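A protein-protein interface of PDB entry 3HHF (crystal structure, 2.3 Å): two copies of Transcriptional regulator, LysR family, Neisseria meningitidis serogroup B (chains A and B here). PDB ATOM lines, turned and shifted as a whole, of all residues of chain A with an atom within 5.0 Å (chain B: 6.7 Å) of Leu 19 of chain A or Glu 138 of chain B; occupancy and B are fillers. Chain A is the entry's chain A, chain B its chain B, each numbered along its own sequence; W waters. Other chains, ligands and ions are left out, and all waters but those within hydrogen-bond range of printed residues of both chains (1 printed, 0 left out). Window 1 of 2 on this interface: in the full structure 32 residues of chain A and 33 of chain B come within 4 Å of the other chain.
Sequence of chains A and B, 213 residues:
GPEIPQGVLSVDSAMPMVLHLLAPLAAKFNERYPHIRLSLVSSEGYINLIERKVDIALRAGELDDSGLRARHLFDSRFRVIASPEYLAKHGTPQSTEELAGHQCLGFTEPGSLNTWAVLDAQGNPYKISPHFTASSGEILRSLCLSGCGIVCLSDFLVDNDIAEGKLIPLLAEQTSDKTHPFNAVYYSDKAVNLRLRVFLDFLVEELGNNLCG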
ATOM      1  N   MET A  15       2.453  19.375   2.404  1.00  0.00           N
ATOM      2  CA  MET A  15       1.459  18.545   1.723  1.00  0.00           C
ATOM      3  C   MET A  15       0.005  18.829   2.145  1.00  0.00           C
ATOM      4  O   MET A  15      -0.856  18.959   1.281  1.00  0.00           O
ATOM      5  CB  MET A  15       1.784  17.055   1.898  1.00  0.00           C
ATOM      6  CG  MET A  15       1.108  16.143   0.874  1.00  0.00           C
ATOM      7  SD  MET A  15       1.586  16.543  -0.986  1.00  0.00           S
ATOM      8  CE  MET A  15       3.315  15.651  -1.150  1.00  0.00           C
ATOM      9  N   PRO A  16      -0.271  18.945   3.462  1.00  0.00           N
ATOM     10  CA  PRO A  16      -1.657  19.173   3.884  1.00  0.00           C
ATOM     11  C   PRO A  16      -2.281  20.464   3.340  1.00  0.00           C
ATOM     12  O   PRO A  16      -3.464  20.486   3.013  1.00  0.00           O
ATOM     13  CB  PRO A  16      -1.556  19.227   5.416  1.00  0.00           C
ATOM     14  CG  PRO A  16      -0.300  18.539   5.746  1.00  0.00           C
ATOM     15  CD  PRO A  16       0.630  18.875   4.623  1.00  0.00           C
ATOM     16  N   MET A  17      -1.491  21.526   3.255  1.00  0.00           N
ATOM     17  CA  MET A  17      -1.956  22.792   2.689  1.00  0.00           C
ATOM     18  C   MET A  17      -2.340  22.622   1.222  1.00  0.00           C
ATOM     19  O   MET A  17      -3.399  23.077   0.800  1.00  0.00           O
ATOM     20  CB  MET A  17      -0.871  23.870   2.845  1.00  0.00           C
ATOM     21  CG  MET A  17      -1.079  25.155   2.030  1.00  0.00           C
ATOM     22  SD  MET A  17      -2.404  26.395   2.784  1.00  0.00           S
ATOM     23  CE  MET A  17      -1.385  27.028   4.334  1.00  0.00           C
ATOM     24  N   VAL A  18      -1.483  21.953   0.454  1.00  0.00           N
ATOM     25  CA  VAL A  18      -1.719  21.754  -0.980  1.00  0.00           C
ATOM     26  C   VAL A  18      -2.976  20.909  -1.228  1.00  0.00           C
ATOM     27  O   VAL A  18      -3.818  21.266  -2.051  1.00  0.00           O
ATOM     28  CB  VAL A  18      -0.522  21.063  -1.694  1.00  0.00           C
ATOM     29  CG1 VAL A  18      -0.661  21.206  -3.200  1.00  0.00           C
ATOM     30  CG2 VAL A  18       0.805  21.640  -1.244  1.00  0.00           C
ATOM     31  N   LEU A  19      -3.099  19.797  -0.508  1.00  0.00           N
ATOM     32  CA  LEU A  19      -4.176  18.832  -0.753  1.00  0.00           C
ATOM     33  C   LEU A  19      -5.552  19.271  -0.258  1.00  0.00           C
ATOM     34  O   LEU A  19      -6.553  19.030  -0.922  1.00  0.00           O
ATOM     35  CB  LEU A  19      -3.833  17.475  -0.134  1.00  0.00           C
ATOM     36  CG  LEU A  19      -2.551  16.793  -0.613  1.00  0.00           C
ATOM     37  CD1 LEU A  19      -2.463  15.403  -0.021  1.00  0.00           C
ATOM     38  CD2 LEU A  19      -2.462  16.742  -2.139  1.00  0.00           C
ATOM     39  N   HIS A  20      -5.609  19.905   0.906  1.00  0.00           N
ATOM     40  CA  HIS A  20      -6.894  20.225   1.535  1.00  0.00           C
ATOM     41  C   HIS A  20      -7.379  21.648   1.274  1.00  0.00           C
ATOM     42  O   HIS A  20      -8.565  21.931   1.437  1.00  0.00           O
ATOM     43  CB  HIS A  20      -6.817  19.954   3.041  1.00  0.00           C
ATOM     44  CG  HIS A  20      -6.542  18.520   3.368  1.00  0.00           C
ATOM     45  ND1 HIS A  20      -7.545  17.589   3.516  1.00  0.00           N
ATOM     46  CD2 HIS A  20      -5.378  17.850   3.537  1.00  0.00           C
ATOM     47  CE1 HIS A  20      -7.012  16.410   3.779  1.00  0.00           C
ATOM     48  NE2 HIS A  20      -5.697  16.539   3.793  1.00  0.00           N
ATOM     49  N   LEU A  21      -6.471  22.529   0.860  1.00  0.00           N
ATOM     50  CA  LEU A  21      -6.757  23.966   0.757  1.00  0.00           C
ATOM     51  C   LEU A  21      -6.521  24.509  -0.654  1.00  0.00           C
ATOM     52  O   LEU A  21      -7.423  25.100  -1.243  1.00  0.00           O
ATOM     53  CB  LEU A  21      -5.923  24.748   1.793  1.00  0.00           C
ATOM     54  CG  LEU A  21      -6.539  25.057   3.177  1.00  0.00           C
ATOM     55  CD1 LEU A  21      -7.555  24.028   3.658  1.00  0.00           C
ATOM     56  CD2 LEU A  21      -5.443  25.227   4.215  1.00  0.00           C
ATOM     57  N   ALA A  23      -5.503  22.728  -3.711  1.00  0.00           N
ATOM     58  CA  ALA A  23      -6.111  21.882  -4.750  1.00  0.00           C
ATOM     59  C   ALA A  23      -7.627  22.109  -4.954  1.00  0.00           C
ATOM     60  O   ALA A  23      -8.076  22.267  -6.095  1.00  0.00           O
ATOM     61  CB  ALA A  23      -5.828  20.410  -4.476  1.00  0.00           C
ATOM     62  N   PRO A  24      -8.424  22.103  -3.863  1.00  0.00           N
ATOM     63  CA  PRO A  24      -9.859  22.407  -3.980  1.00  0.00           C
ATOM     64  C   PRO A  24     -10.194  23.764  -4.618  1.00  0.00           C
ATOM     65  O   PRO A  24     -11.190  23.868  -5.330  1.00  0.00           O
ATOM     66  CB  PRO A  24     -10.348  22.362  -2.527  1.00  0.00           C
ATOM     67  CG  PRO A  24      -9.399  21.475  -1.841  1.00  0.00           C
ATOM     68  CD  PRO A  24      -8.067  21.762  -2.476  1.00  0.00           C
ATOM     69  N   GLU A 138       0.286  14.873   6.691  1.00  0.00           N
ATOM     70  CA  GLU A 138      -0.617  14.151   5.798  1.00  0.00           C
ATOM     71  C   GLU A 138      -0.506  12.643   6.012  1.00  0.00           C
ATOM     72  O   GLU A 138      -1.503  11.935   5.942  1.00  0.00           O
ATOM     73  CB  GLU A 138      -0.337  14.521   4.334  1.00  0.00           C
ATOM     74  CG  GLU A 138      -1.431  14.089   3.356  1.00  0.00           C
ATOM     75  CD  GLU A 138      -2.773  14.766   3.616  1.00  0.00           C
ATOM     76  OE1 GLU A 138      -2.788  15.993   3.844  1.00  0.00           O
ATOM     77  OE2 GLU A 138      -3.816  14.075   3.593  1.00  0.00           O
ATOM     78  N   MET B  15       4.816  10.113  -1.834  1.00  0.00           N
ATOM     79  CA  MET B  15       3.606  10.362  -1.050  1.00  0.00           C
ATOM     80  C   MET B  15       2.441   9.404  -1.360  1.00  0.00           C
ATOM     81  O   MET B  15       1.873   8.830  -0.435  1.00  0.00           O
ATOM     82  CB  MET B  15       3.164  11.833  -1.192  1.00  0.00           C
ATOM     83  CG  MET B  15       2.261  12.341  -0.069  1.00  0.00           C
ATOM     84  SD  MET B  15       3.039  12.182   1.725  1.00  0.00           S
ATOM     85  CE  MET B  15       4.043  13.854   1.853  1.00  0.00           C
ATOM     86  N   PRO B  16       2.074   9.230  -2.646  1.00  0.00           N
ATOM     87  CA  PRO B  16       0.950   8.328  -2.913  1.00  0.00           C
ATOM     88  C   PRO B  16       1.138   6.874  -2.434  1.00  0.00           C
ATOM     89  O   PRO B  16       0.160   6.227  -2.047  1.00  0.00           O
ATOM     90  CB  PRO B  16       0.777   8.405  -4.440  1.00  0.00           C
ATOM     91  CG  PRO B  16       1.992   9.025  -4.959  1.00  0.00           C
ATOM     92  CD  PRO B  16       2.588   9.849  -3.879  1.00  0.00           C
ATOM     93  N   MET B  17       2.370   6.374  -2.445  1.00  0.00           N
ATOM     94  CA  MET B  17       2.663   5.037  -1.919  1.00  0.00           C
ATOM     95  C   MET B  17       2.436   4.967  -0.400  1.00  0.00           C
ATOM     96  O   MET B  17       1.891   3.987   0.103  1.00  0.00           O
ATOM     97  CB  MET B  17       4.096   4.630  -2.284  1.00  0.00           C
ATOM     98  CG  MET B  17       4.713   3.503  -1.442  1.00  0.00           C
ATOM     99  SD  MET B  17       4.235   1.691  -2.017  1.00  0.00           S
ATOM    100  CE  MET B  17       5.342   1.607  -3.636  1.00  0.00           C
ATOM    101  N   LEU B  19       0.496   6.999   1.551  1.00  0.00           N
ATOM    102  CA  LEU B  19      -0.884   7.283   1.956  1.00  0.00           C
ATOM    103  C   LEU B  19      -1.886   6.226   1.510  1.00  0.00           C
ATOM    104  O   LEU B  19      -2.847   5.963   2.224  1.00  0.00           O
ATOM    105  CB  LEU B  19      -1.331   8.647   1.412  1.00  0.00           C
ATOM    106  CG  LEU B  19      -0.497   9.862   1.817  1.00  0.00           C
ATOM    107  CD1 LEU B  19      -1.129  11.129   1.260  1.00  0.00           C
ATOM    108  CD2 LEU B  19      -0.354   9.927   3.327  1.00  0.00           C
ATOM    109  N   HIS B  20      -1.679   5.645   0.329  1.00  0.00           N
ATOM    110  CA  HIS B  20      -2.646   4.716  -0.252  1.00  0.00           C
ATOM    111  C   HIS B  20      -2.310   3.249  -0.030  1.00  0.00           C
ATOM    112  O   HIS B  20      -3.198   2.402  -0.113  1.00  0.00           O
ATOM    113  CB  HIS B  20      -2.819   4.997  -1.747  1.00  0.00           C
ATOM    114  CG  HIS B  20      -3.358   6.361  -2.031  1.00  0.00           C
ATOM    115  ND1 HIS B  20      -4.708   6.633  -2.063  1.00  0.00           N
ATOM    116  CD2 HIS B  20      -2.732   7.540  -2.254  1.00  0.00           C
ATOM    117  CE1 HIS B  20      -4.889   7.919  -2.304  1.00  0.00           C
ATOM    118  NE2 HIS B  20      -3.706   8.492  -2.422  1.00  0.00           N
ATOM    119  N   PHE B 107       3.393  16.580 -14.208  1.00  0.00           N
ATOM    120  CA  PHE B 107       4.465  16.744 -13.233  1.00  0.00           C
ATOM    121  C   PHE B 107       5.390  17.876 -13.656  1.00  0.00           C
ATOM    122  O   PHE B 107       5.653  18.059 -14.847  1.00  0.00           O
ATOM    123  CB  PHE B 107       5.291  15.457 -13.101  1.00  0.00           C
ATOM    124  CG  PHE B 107       4.581  14.341 -12.374  1.00  0.00           C
ATOM    125  CD1 PHE B 107       3.681  13.523 -13.040  1.00  0.00           C
ATOM    126  CD2 PHE B 107       4.821  14.107 -11.024  1.00  0.00           C
ATOM    127  CE1 PHE B 107       3.029  12.494 -12.377  1.00  0.00           C
ATOM    128  CE2 PHE B 107       4.175  13.083 -10.358  1.00  0.00           C
ATOM    129  CZ  PHE B 107       3.276  12.272 -11.039  1.00  0.00           C
ATOM    130  N   SER B 135       4.582  18.671  -8.016  1.00  0.00           N
ATOM    131  CA  SER B 135       5.754  17.893  -7.633  1.00  0.00           C
ATOM    132  C   SER B 135       5.423  16.429  -7.300  1.00  0.00           C
ATOM    133  O   SER B 135       6.317  15.588  -7.261  1.00  0.00           O
ATOM    134  CB  SER B 135       6.442  18.555  -6.437  1.00  0.00           C
ATOM    135  OG  SER B 135       5.555  18.689  -5.338  1.00  0.00           O
ATOM    136  N   SER B 136       4.145  16.131  -7.067  1.00  0.00           N
ATOM    137  CA  SER B 136       3.723  14.820  -6.583  1.00  0.00           C
ATOM    138  C   SER B 136       2.453  14.369  -7.288  1.00  0.00           C
ATOM    139  O   SER B 136       1.611  15.195  -7.651  1.00  0.00           O
ATOM    140  CB  SER B 136       3.486  14.881  -5.066  1.00  0.00           C
ATOM    141  OG  SER B 136       2.881  13.698  -4.566  1.00  0.00           O
ATOM    142  N   GLY B 137       2.327  13.056  -7.472  1.00  0.00           N
ATOM    143  CA  GLY B 137       1.118  12.447  -8.030  1.00  0.00           C
ATOM    144  C   GLY B 137      -0.087  12.570  -7.107  1.00  0.00           C
ATOM    145  O   GLY B 137      -1.236  12.535  -7.561  1.00  0.00           O
ATOM    146  N   GLU B 138       0.175  12.719  -5.809  1.00  0.00           N
ATOM    147  CA  GLU B 138      -0.886  12.970  -4.837  1.00  0.00           C
ATOM    148  C   GLU B 138      -1.520  14.345  -5.051  1.00  0.00           C
ATOM    149  O   GLU B 138      -2.733  14.494  -4.937  1.00  0.00           O
ATOM    150  CB  GLU B 138      -0.349  12.862  -3.413  1.00  0.00           C
ATOM    151  CG  GLU B 138      -1.429  12.726  -2.363  1.00  0.00           C
ATOM    152  CD  GLU B 138      -2.149  11.385  -2.412  1.00  0.00           C
ATOM    153  OE1 GLU B 138      -1.507  10.360  -2.730  1.00  0.00           O
ATOM    154  OE2 GLU B 138      -3.360  11.357  -2.114  1.00  0.00           O
ATOM    155  N   ILE B 139      -0.699  15.345  -5.362  1.00  0.00           N
ATOM    156  CA  ILE B 139      -1.208  16.683  -5.682  1.00  0.00           C
ATOM    157  C   ILE B 139      -2.067  16.627  -6.950  1.00  0.00           C
ATOM    158  O   ILE B 139      -3.119  17.259  -7.024  1.00  0.00           O
ATOM    159  CB  ILE B 139      -0.070  17.735  -5.847  1.00  0.00           C
ATOM    160  CG1 ILE B 139       0.798  17.822  -4.574  1.00  0.00           C
ATOM    161  CG2 ILE B 139      -0.658  19.111  -6.173  1.00  0.00           C
ATOM    162  CD1 ILE B 139       2.017  18.736  -4.701  1.00  0.00           C
ATOM    163  N   LEU B 140      -1.624  15.850  -7.936  1.00  0.00           N
ATOM    164  CA  LEU B 140      -2.369  15.680  -9.184  1.00  0.00           C
ATOM    165  C   LEU B 140      -3.718  14.995  -8.941  1.00  0.00           C
ATOM    166  O   LEU B 140      -4.720  15.353  -9.570  1.00  0.00           O
ATOM    167  CB  LEU B 140      -1.546  14.888 -10.214  1.00  0.00           C
ATOM    168  CG  LEU B 140      -0.329  15.585 -10.826  1.00  0.00           C
ATOM    169  CD1 LEU B 140       0.423  14.647 -11.752  1.00  0.00           C
ATOM    170  CD2 LEU B 140      -0.742  16.839 -11.569  1.00  0.00           C
ATOM    171  N   ARG B 141      -3.748  14.017  -8.039  1.00  0.00           N
ATOM    172  CA  ARG B 141      -5.003  13.362  -7.661  1.00  0.00           C
ATOM    173  C   ARG B 141      -6.025  14.356  -7.096  1.00  0.00           C
ATOM    174  O   ARG B 141      -7.199  14.309  -7.450  1.00  0.00           O
ATOM    175  CB  ARG B 141      -4.746  12.239  -6.648  1.00  0.00           C
ATOM    176  CG  ARG B 141      -6.004  11.504  -6.217  1.00  0.00           C
ATOM    177  CD  ARG B 141      -5.693  10.333  -5.313  1.00  0.00           C
ATOM    178  NE  ARG B 141      -6.864   9.931  -4.537  1.00  0.00           N
ATOM    179  CZ  ARG B 141      -7.297  10.562  -3.445  1.00  0.00           C
ATOM    180  NH1 ARG B 141      -6.646  11.619  -2.965  1.00  0.00           N
ATOM    181  NH2 ARG B 141      -8.386  10.123  -2.821  1.00  0.00           N
ATOM    182  N   SER B 142      -5.574  15.246  -6.216  1.00  0.00           N
ATOM    183  CA  SER B 142      -6.441  16.261  -5.620  1.00  0.00           C
ATOM    184  C   SER B 142      -6.940  17.269  -6.645  1.00  0.00           C
ATOM    185  O   SER B 142      -8.122  17.610  -6.655  1.00  0.00           O
ATOM    186  CB  SER B 142      -5.719  16.996  -4.487  1.00  0.00           C
ATOM    187  OG  SER B 142      -5.476  16.133  -3.392  1.00  0.00           O
ATOM    188  N   LEU B 143      -6.044  17.755  -7.497  1.00  0.00           N
ATOM    189  CA  LEU B 143      -6.441  18.675  -8.568  1.00  0.00           C
ATOM    190  C   LEU B 143      -7.515  18.032  -9.453  1.00  0.00           C
ATOM    191  O   LEU B 143      -8.535  18.649  -9.753  1.00  0.00           O
ATOM    192  CB  LEU B 143      -5.231  19.096  -9.414  1.00  0.00           C
ATOM    193  CG  LEU B 143      -4.192  19.983  -8.722  1.00  0.00           C
ATOM    194  CD1 LEU B 143      -2.947  20.166  -9.591  1.00  0.00           C
ATOM    195  CD2 LEU B 143      -4.788  21.327  -8.339  1.00  0.00           C
ATOM    196  N   SER B 146     -10.840  17.784  -7.760  1.00  0.00           N
ATOM    197  CA  SER B 146     -11.421  19.134  -7.671  1.00  0.00           C
ATOM    198  C   SER B 146     -11.891  19.721  -9.016  1.00  0.00           C
ATOM    199  O   SER B 146     -12.416  20.835  -9.051  1.00  0.00           O
ATOM    200  CB  SER B 146     -10.411  20.079  -7.019  1.00  0.00           C
ATOM    201  OG  SER B 146      -9.907  19.508  -5.821  1.00  0.00           O
ATOM    202  N   LEU B 153      -2.377   8.659 -13.798  1.00  0.00           N
ATOM    203  CA  LEU B 153      -1.771   8.246 -12.531  1.00  0.00           C
ATOM    204  C   LEU B 153      -1.876   6.740 -12.339  1.00  0.00           C
ATOM    205  O   LEU B 153      -2.671   6.073 -12.996  1.00  0.00           O
ATOM    206  CB  LEU B 153      -2.456   8.944 -11.350  1.00  0.00           C
ATOM    207  CG  LEU B 153      -2.489  10.473 -11.334  1.00  0.00           C
ATOM    208  CD1 LEU B 153      -3.450  10.960 -10.271  1.00  0.00           C
ATOM    209  CD2 LEU B 153      -1.083  11.042 -11.128  1.00  0.00           C
ATOM    210  N   LEU B 157      -3.409   4.697  -6.842  1.00  0.00           N
ATOM    211  CA  LEU B 157      -3.691   6.057  -6.414  1.00  0.00           C
ATOM    212  C   LEU B 157      -5.175   6.393  -6.625  1.00  0.00           C
ATOM    213  O   LEU B 157      -5.791   7.036  -5.786  1.00  0.00           O
ATOM    214  CB  LEU B 157      -2.782   7.024  -7.190  1.00  0.00           C
ATOM    215  CG  LEU B 157      -2.770   8.528  -6.905  1.00  0.00           C
ATOM    216  CD1 LEU B 157      -2.724   8.848  -5.417  1.00  0.00           C
ATOM    217  CD2 LEU B 157      -1.578   9.162  -7.614  1.00  0.00           C
HETATM  218  O   HOH W   1      -8.311  17.173  -1.973  1.00  0.00           O
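The side-chain hydroxyl (OG) of Ser 146 of chain B lies within hydrogen-bond range of the backbone carbonyl oxygen (O) of Ala 23 of chain A (3.3 Å).
The backbone carbonyl oxygen (O) of Val 18 of chain A sits at hydrogen-bond distance from the backbone NH (N) of Ala 23 of chain A. A ring nitrogen (NE2) of His 20 of chain B lies within hydrogen-bond range of the side-chain carboxylate (OE1) of Glu 138 of chain B (2.9 Å). O of Ser 142 of chain B lies within hydrogen-bond range of OG of Ser 146 of chain B, at 2.7 Å. NH1 of Arg 141 of chain B lies within salt-bridge range of OE2 of Glu 138 of chain B, 3.4 Å away. The side-chain carboxylate (OE1) of Glu 138 of chain A lies within hydrogen-bond range of a ring nitrogen (NE2) of His 20 of chain A (3.0 Å). The side-chain hydroxyl (OG) of Ser 136 of chain B lies within hydrogen-bond range of the backbone NH (N) of Glu 138 of chain B.
CE of Met 15 of chain A touches CE of Met 15 of chain B, 3.6 Å away. CE of Met 15 of chain A touches OG of Ser 136 of chain B, at 3.96 Å. SD of Met 15 of chain A touches CG1 of Ile 139 of chain B, at 3.9 Å. CG2 of Ile 139 of chain B touches CG1 of Val 18 of chain A (3.6 Å). O of Glu 138 of chain B touches CD2 of Leu 19 of chain A (3.6 Å). Ile 139 of chain B touches Leu 19 of chain A. Leu 19 of chain A touches Ser 142 of chain B. Ser 142 of chain B touches Ala 23 of chain A. Pro 24 of chain A touches Ser 146 of chain B. Leu 19 of chain B touches Glu 138 of chain A.
Leu 19 of chain A touches just these residues of chain B: Glu 138, Ile 139 and Ser 142. Of the printed residues of chain A, Glu 138 of chain B touches Leu 19 (3.6 Å). Printed residues of chain A within 4 Å of Met 15 of chain B: Met 15. Of the printed residues of chain A, Ser 136 of chain B touches Met 15. Printed residues of chain B within 4 Å of Val 18 of chain A: Ile 139. Of the printed residues of chain A, Leu 143 of chain B touches Ala 23 (3.9 Å). Printed residues of chain A within 4 Å of Ser 142 of chain B: Leu 19 and Ala 23. Arg 141 of chain B touches none of the printed residues of chain A.
Met 15 of chain A touches its own counterpart, Met 15 of chain B. Leu 19 of chain A touches Glu 138 of chain B, and with the chains exchanged Glu 138 of chain A touches Leu 19 of chain B. 6 positions are printed for both chains.
Water W1 bridges the backbone carbonyl oxygen (O) of Leu 19 of chain A (2.8 Å) and the side-chain hydroxyl (OG) of Ser 142 of chain B (3.3 Å).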
